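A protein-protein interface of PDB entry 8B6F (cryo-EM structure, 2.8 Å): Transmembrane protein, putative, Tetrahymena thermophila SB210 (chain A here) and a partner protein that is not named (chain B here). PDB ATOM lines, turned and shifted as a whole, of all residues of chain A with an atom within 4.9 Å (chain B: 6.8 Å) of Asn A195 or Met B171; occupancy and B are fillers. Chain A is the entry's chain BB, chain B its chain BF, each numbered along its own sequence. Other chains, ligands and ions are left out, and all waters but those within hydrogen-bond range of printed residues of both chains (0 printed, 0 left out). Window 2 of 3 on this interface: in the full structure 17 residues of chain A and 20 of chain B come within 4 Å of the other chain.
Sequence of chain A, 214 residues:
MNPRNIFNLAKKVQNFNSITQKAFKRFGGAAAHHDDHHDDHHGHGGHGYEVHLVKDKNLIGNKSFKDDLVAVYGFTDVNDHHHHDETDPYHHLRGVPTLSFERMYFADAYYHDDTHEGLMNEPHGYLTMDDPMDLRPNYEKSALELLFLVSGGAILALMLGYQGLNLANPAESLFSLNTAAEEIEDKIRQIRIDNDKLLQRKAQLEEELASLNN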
ATOM      1  N   ILE A 188      15.626  -2.174 -17.658  1.00  0.00           N
ATOM      2  CA  ILE A 188      15.462  -2.708 -16.310  1.00  0.00           C
ATOM      3  C   ILE A 188      14.643  -1.748 -15.457  1.00  0.00           C
ATOM      4  O   ILE A 188      13.810  -2.171 -14.648  1.00  0.00           O
ATOM      5  CB  ILE A 188      16.834  -3.007 -15.677  1.00  0.00           C
ATOM      6  CG1 ILE A 188      17.470  -4.221 -16.357  1.00  0.00           C
ATOM      7  CG2 ILE A 188      16.693  -3.263 -14.178  1.00  0.00           C
ATOM      8  CD1 ILE A 188      18.913  -4.463 -15.963  1.00  0.00           C
ATOM      9  N   ILE A 191      11.061  -2.250 -16.420  1.00  0.00           N
ATOM     10  CA  ILE A 191      10.563  -3.504 -15.862  1.00  0.00           C
ATOM     11  C   ILE A 191      10.282  -3.348 -14.375  1.00  0.00           C
ATOM     12  O   ILE A 191       9.288  -3.871 -13.858  1.00  0.00           O
ATOM     13  CB  ILE A 191      11.559  -4.647 -16.137  1.00  0.00           C
ATOM     14  CG1 ILE A 191      11.579  -4.976 -17.634  1.00  0.00           C
ATOM     15  CG2 ILE A 191      11.195  -5.889 -15.323  1.00  0.00           C
ATOM     16  CD1 ILE A 191      12.654  -5.963 -18.039  1.00  0.00           C
ATOM     17  N   ARG A 192      11.155  -2.636 -13.660  1.00  0.00           N
ATOM     18  CA  ARG A 192      10.906  -2.387 -12.245  1.00  0.00           C
ATOM     19  C   ARG A 192       9.609  -1.616 -12.043  1.00  0.00           C
ATOM     20  O   ARG A 192       8.825  -1.931 -11.142  1.00  0.00           O
ATOM     21  CB  ARG A 192      12.073  -1.614 -11.633  1.00  0.00           C
ATOM     22  CG  ARG A 192      13.331  -2.432 -11.426  1.00  0.00           C
ATOM     23  CD  ARG A 192      14.407  -1.597 -10.750  1.00  0.00           C
ATOM     24  NE  ARG A 192      15.644  -2.343 -10.566  1.00  0.00           N
ATOM     25  CZ  ARG A 192      16.756  -1.835 -10.055  1.00  0.00           C
ATOM     26  NH1 ARG A 192      16.824  -0.574  -9.661  1.00  0.00           N
ATOM     27  NH2 ARG A 192      17.828  -2.612  -9.936  1.00  0.00           N
ATOM     28  N   ILE A 193       9.368  -0.598 -12.868  1.00  0.00           N
ATOM     29  CA  ILE A 193       8.141   0.183 -12.739  1.00  0.00           C
ATOM     30  C   ILE A 193       6.926  -0.708 -12.963  1.00  0.00           C
ATOM     31  O   ILE A 193       5.942  -0.646 -12.216  1.00  0.00           O
ATOM     32  CB  ILE A 193       8.165   1.373 -13.716  1.00  0.00           C
ATOM     33  CG1 ILE A 193       9.253   2.368 -13.304  1.00  0.00           C
ATOM     34  CG2 ILE A 193       6.809   2.064 -13.757  1.00  0.00           C
ATOM     35  CD1 ILE A 193       9.511   3.462 -14.323  1.00  0.00           C
ATOM     36  N   ASP A 194       6.971  -1.547 -14.002  1.00  0.00           N
ATOM     37  CA  ASP A 194       5.839  -2.424 -14.288  1.00  0.00           C
ATOM     38  C   ASP A 194       5.601  -3.407 -13.151  1.00  0.00           C
ATOM     39  O   ASP A 194       4.457  -3.629 -12.741  1.00  0.00           O
ATOM     40  CB  ASP A 194       6.074  -3.174 -15.597  1.00  0.00           C
ATOM     41  CG  ASP A 194       6.232  -2.243 -16.780  1.00  0.00           C
ATOM     42  OD1 ASP A 194       6.201  -1.011 -16.576  1.00  0.00           O
ATOM     43  OD2 ASP A 194       6.384  -2.743 -17.915  1.00  0.00           O
ATOM     44  N   ASN A 195       6.670  -4.014 -12.634  1.00  0.00           N
ATOM     45  CA  ASN A 195       6.518  -4.956 -11.532  1.00  0.00           C
ATOM     46  C   ASN A 195       5.955  -4.268 -10.299  1.00  0.00           C
ATOM     47  O   ASN A 195       5.110  -4.831  -9.595  1.00  0.00           O
ATOM     48  CB  ASN A 195       7.863  -5.611 -11.211  1.00  0.00           C
ATOM     49  CG  ASN A 195       8.381  -6.464 -12.349  1.00  0.00           C
ATOM     50  OD1 ASN A 195       7.841  -6.441 -13.454  1.00  0.00           O
ATOM     51  ND2 ASN A 195       9.438  -7.223 -12.084  1.00  0.00           N
ATOM     52  N   ASP A 196       6.416  -3.048 -10.018  1.00  0.00           N
ATOM     53  CA  ASP A 196       5.888  -2.305  -8.880  1.00  0.00           C
ATOM     54  C   ASP A 196       4.407  -2.002  -9.059  1.00  0.00           C
ATOM     55  O   ASP A 196       3.628  -2.107  -8.105  1.00  0.00           O
ATOM     56  CB  ASP A 196       6.677  -1.012  -8.685  1.00  0.00           C
ATOM     57  CG  ASP A 196       6.255  -0.258  -7.440  1.00  0.00           C
ATOM     58  OD1 ASP A 196       6.610  -0.698  -6.327  1.00  0.00           O
ATOM     59  OD2 ASP A 196       5.566   0.776  -7.572  1.00  0.00           O
ATOM     60  N   LYS A 197       3.994  -1.629 -10.272  1.00  0.00           N
ATOM     61  CA  LYS A 197       2.578  -1.374 -10.514  1.00  0.00           C
ATOM     62  C   LYS A 197       1.747  -2.622 -10.251  1.00  0.00           C
ATOM     63  O   LYS A 197       0.700  -2.559  -9.598  1.00  0.00           O
ATOM     64  CB  LYS A 197       2.368  -0.883 -11.947  1.00  0.00           C
ATOM     65  CG  LYS A 197       2.726   0.580 -12.162  1.00  0.00           C
ATOM     66  CD  LYS A 197       2.341   1.041 -13.559  1.00  0.00           C
ATOM     67  CE  LYS A 197       2.468   2.549 -13.702  1.00  0.00           C
ATOM     68  NZ  LYS A 197       3.863   3.024 -13.511  1.00  0.00           N
ATOM     69  N   LEU A 198       2.197  -3.769 -10.759  1.00  0.00           N
ATOM     70  CA  LEU A 198       1.454  -5.005 -10.544  1.00  0.00           C
ATOM     71  C   LEU A 198       1.389  -5.359  -9.064  1.00  0.00           C
ATOM     72  O   LEU A 198       0.335  -5.765  -8.561  1.00  0.00           O
ATOM     73  CB  LEU A 198       2.090  -6.141 -11.342  1.00  0.00           C
ATOM     74  CG  LEU A 198       1.487  -6.391 -12.727  1.00  0.00           C
ATOM     75  CD1 LEU A 198       1.574  -5.144 -13.591  1.00  0.00           C
ATOM     76  CD2 LEU A 198       2.176  -7.562 -13.405  1.00  0.00           C
ATOM     77  N   LEU A 199       2.506  -5.215  -8.349  1.00  0.00           N
ATOM     78  CA  LEU A 199       2.515  -5.527  -6.923  1.00  0.00           C
ATOM     79  C   LEU A 199       1.589  -4.600  -6.149  1.00  0.00           C
ATOM     80  O   LEU A 199       0.884  -5.038  -5.232  1.00  0.00           O
ATOM     81  CB  LEU A 199       3.939  -5.443  -6.374  1.00  0.00           C
ATOM     82  CG  LEU A 199       4.917  -6.517  -6.858  1.00  0.00           C
ATOM     83  CD1 LEU A 199       6.314  -6.233  -6.337  1.00  0.00           C
ATOM     84  CD2 LEU A 199       4.464  -7.903  -6.430  1.00  0.00           C
ATOM     85  N   ARG B 166      22.230 -11.890 -12.077  1.00  0.00           N
ATOM     86  CA  ARG B 166      22.280 -10.458 -11.802  1.00  0.00           C
ATOM     87  C   ARG B 166      21.077  -9.739 -12.398  1.00  0.00           C
ATOM     88  O   ARG B 166      20.463  -8.893 -11.741  1.00  0.00           O
ATOM     89  CB  ARG B 166      23.580  -9.868 -12.349  1.00  0.00           C
ATOM     90  CG  ARG B 166      23.706  -8.364 -12.165  1.00  0.00           C
ATOM     91  CD  ARG B 166      25.013  -7.852 -12.732  1.00  0.00           C
ATOM     92  NE  ARG B 166      26.167  -8.386 -12.017  1.00  0.00           N
ATOM     93  CZ  ARG B 166      26.732  -7.817 -10.960  1.00  0.00           C
ATOM     94  NH1 ARG B 166      26.271  -6.685 -10.454  1.00  0.00           N
ATOM     95  NH2 ARG B 166      27.789  -8.396 -10.401  1.00  0.00           N
ATOM     96  N   LEU B 167      20.721 -10.067 -13.641  1.00  0.00           N
ATOM     97  CA  LEU B 167      19.566  -9.434 -14.269  1.00  0.00           C
ATOM     98  C   LEU B 167      18.282  -9.772 -13.526  1.00  0.00           C
ATOM     99  O   LEU B 167      17.417  -8.907 -13.345  1.00  0.00           O
ATOM    100  CB  LEU B 167      19.467  -9.858 -15.732  1.00  0.00           C
ATOM    101  CG  LEU B 167      20.552  -9.324 -16.670  1.00  0.00           C
ATOM    102  CD1 LEU B 167      20.374  -9.910 -18.055  1.00  0.00           C
ATOM    103  CD2 LEU B 167      20.536  -7.803 -16.727  1.00  0.00           C
ATOM    104  N   LEU B 168      18.132 -11.024 -13.095  1.00  0.00           N
ATOM    105  CA  LEU B 168      16.947 -11.396 -12.330  1.00  0.00           C
ATOM    106  C   LEU B 168      16.852 -10.586 -11.045  1.00  0.00           C
ATOM    107  O   LEU B 168      15.789 -10.053 -10.710  1.00  0.00           O
ATOM    108  CB  LEU B 168      16.973 -12.894 -12.019  1.00  0.00           C
ATOM    109  CG  LEU B 168      16.173 -13.807 -12.945  1.00  0.00           C
ATOM    110  CD1 LEU B 168      14.687 -13.500 -12.832  1.00  0.00           C
ATOM    111  CD2 LEU B 168      16.654 -13.656 -14.379  1.00  0.00           C
ATOM    112  N   LYS B 169      17.962 -10.471 -10.315  1.00  0.00           N
ATOM    113  CA  LYS B 169      17.946  -9.716  -9.067  1.00  0.00           C
ATOM    114  C   LYS B 169      17.631  -8.246  -9.317  1.00  0.00           C
ATOM    115  O   LYS B 169      16.850  -7.637  -8.578  1.00  0.00           O
ATOM    116  CB  LYS B 169      19.285  -9.868  -8.347  1.00  0.00           C
ATOM    117  CG  LYS B 169      19.334  -9.184  -6.993  1.00  0.00           C
ATOM    118  CD  LYS B 169      20.532  -9.639  -6.175  1.00  0.00           C
ATOM    119  CE  LYS B 169      21.847  -9.298  -6.864  1.00  0.00           C
ATOM    120  NZ  LYS B 169      23.022  -9.697  -6.039  1.00  0.00           N
ATOM    121  N   GLU B 170      18.228  -7.660 -10.357  1.00  0.00           N
ATOM    122  CA  GLU B 170      17.972  -6.256 -10.663  1.00  0.00           C
ATOM    123  C   GLU B 170      16.508  -6.024 -11.014  1.00  0.00           C
ATOM    124  O   GLU B 170      15.904  -5.040 -10.571  1.00  0.00           O
ATOM    125  CB  GLU B 170      18.873  -5.798 -11.810  1.00  0.00           C
ATOM    126  CG  GLU B 170      20.350  -5.762 -11.461  1.00  0.00           C
ATOM    127  CD  GLU B 170      20.677  -4.715 -10.419  1.00  0.00           C
ATOM    128  OE1 GLU B 170      19.782  -3.917 -10.074  1.00  0.00           O
ATOM    129  OE2 GLU B 170      21.830  -4.690  -9.942  1.00  0.00           O
ATOM    130  N   MET B 171      15.921  -6.917 -11.811  1.00  0.00           N
ATOM    131  CA  MET B 171      14.509  -6.791 -12.153  1.00  0.00           C
ATOM    132  C   MET B 171      13.626  -6.914 -10.916  1.00  0.00           C
ATOM    133  O   MET B 171      12.667  -6.152 -10.749  1.00  0.00           O
ATOM    134  CB  MET B 171      14.126  -7.845 -13.191  1.00  0.00           C
ATOM    135  CG  MET B 171      14.779  -7.637 -14.550  1.00  0.00           C
ATOM    136  SD  MET B 171      14.450  -8.988 -15.697  1.00  0.00           S
ATOM    137  CE  MET B 171      15.378  -8.449 -17.129  1.00  0.00           C
ATOM    138  N   GLN B 172      13.936  -7.866 -10.034  1.00  0.00           N
ATOM    139  CA  GLN B 172      13.135  -8.051  -8.829  1.00  0.00           C
ATOM    140  C   GLN B 172      13.259  -6.877  -7.863  1.00  0.00           C
ATOM    141  O   GLN B 172      12.349  -6.647  -7.060  1.00  0.00           O
ATOM    142  CB  GLN B 172      13.539  -9.350  -8.128  1.00  0.00           C
ATOM    143  CG  GLN B 172      13.245 -10.613  -8.929  1.00  0.00           C
ATOM    144  CD  GLN B 172      11.776 -10.763  -9.280  1.00  0.00           C
ATOM    145  OE1 GLN B 172      11.430 -11.090 -10.414  1.00  0.00           O
ATOM    146  NE2 GLN B 172      10.905 -10.530  -8.303  1.00  0.00           N
ATOM    147  N   LYS B 173      14.361  -6.131  -7.914  1.00  0.00           N
ATOM    148  CA  LYS B 173      14.499  -4.975  -7.041  1.00  0.00           C
ATOM    149  C   LYS B 173      13.393  -3.962  -7.332  1.00  0.00           C
ATOM    150  O   LYS B 173      12.934  -3.841  -8.472  1.00  0.00           O
ATOM    151  CB  LYS B 173      15.866  -4.317  -7.225  1.00  0.00           C
ATOM    152  CG  LYS B 173      17.004  -5.023  -6.502  1.00  0.00           C
ATOM    153  CD  LYS B 173      18.325  -4.297  -6.712  1.00  0.00           C
ATOM    154  CE  LYS B 173      19.474  -5.042  -6.053  1.00  0.00           C
ATOM    155  NZ  LYS B 173      20.786  -4.384  -6.315  1.00  0.00           N
ATOM    156  N   PRO B 174      12.937  -3.228  -6.321  1.00  0.00           N
ATOM    157  CA  PRO B 174      11.865  -2.255  -6.535  1.00  0.00           C
ATOM    158  C   PRO B 174      12.407  -0.965  -7.123  1.00  0.00           C
ATOM    159  O   PRO B 174      13.623  -0.720  -7.090  1.00  0.00           O
ATOM    160  CB  PRO B 174      11.306  -2.036  -5.124  1.00  0.00           C
ATOM    161  CG  PRO B 174      12.481  -2.243  -4.240  1.00  0.00           C
ATOM    162  CD  PRO B 174      13.337  -3.296  -4.903  1.00  0.00           C
ATOM    163  N   PRO B 175      11.539  -0.110  -7.663  1.00  0.00           N
ATOM    164  CA  PRO B 175      12.018   1.148  -8.250  1.00  0.00           C
ATOM    165  C   PRO B 175      12.653   2.050  -7.204  1.00  0.00           C
ATOM    166  O   PRO B 175      12.278   2.039  -6.030  1.00  0.00           O
ATOM    167  CB  PRO B 175      10.746   1.780  -8.833  1.00  0.00           C
ATOM    168  CG  PRO B 175       9.764   0.668  -8.936  1.00  0.00           C
ATOM    169  CD  PRO B 175      10.084  -0.265  -7.814  1.00  0.00           C
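Of the 10 printed residues of chain B, 6 touch a printed residue of chain A.
Printed residues of chain B that touch a printed residue of chain A: Leu B167, Glu B170, Met B171, Lys B173, Pro B174 and Pro B175.
Hydrophobic or aromatic side chains of chain A within 4 Å of the printed part of chain B: Ile A188 and Ile A191.
Among the printed residues, 9 pairs touch across the chains.
Among the printed residues, Asp or Glu carboxylates within 4 Å of a Lys or Arg side-chain nitrogen of the other chain: Arg A192 with Glu B170 (2.4 Å).
Among the printed residues, pairs that only touch across the chains: Arg A192 with Lys B173, Asp A196 with Pro B175, Arg A192 with Pro B175, Asn A195 with Met B171, Ile A188 with Leu B167, Ile A191 with Met B171, Arg A192 with Met B171 and Arg A192 with Pro B174.
The backbone carbonyl oxygen of Ile A191 lies close to the side-chain amide oxygen of Asn A195 (3.0 Å).
OE2 of Glu B170 lies within salt-bridge range of NZ of Lys B173 (3.8 Å).
NE of Arg A192 is in hydrogen-bond range of O of Glu B170, at 2.7 Å.
Of the printed residues of chain B, Ile A188 touches Leu B167 (3.8 Å).
Asn A195 touches just one residue of chain B: Met B171.
Of the printed residues of chain B, Asp A196 touches Pro B175 (3.5 Å).
Lys A197 touches none of the printed residues of chain B.
Arg B166 touches none of the printed residues of chain A.
Printed residues of chain A within 4 Å of Glu B170: Arg A192.
Of chain A, only Ile A191, Arg A192 and Asn A195 come within 4 Å of Met B171.
Of the printed residues of chain A, Lys B173 touches Arg A192.
Of the printed residues of chain A, Pro B174 touches Arg A192.
The nearest residue of chain B that does not touch Asn A195 is Gln B172 (4.7 Å).
The nearest printed residue of chain A that does not touch Glu B170 is Ile A188 (4.1 Å).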
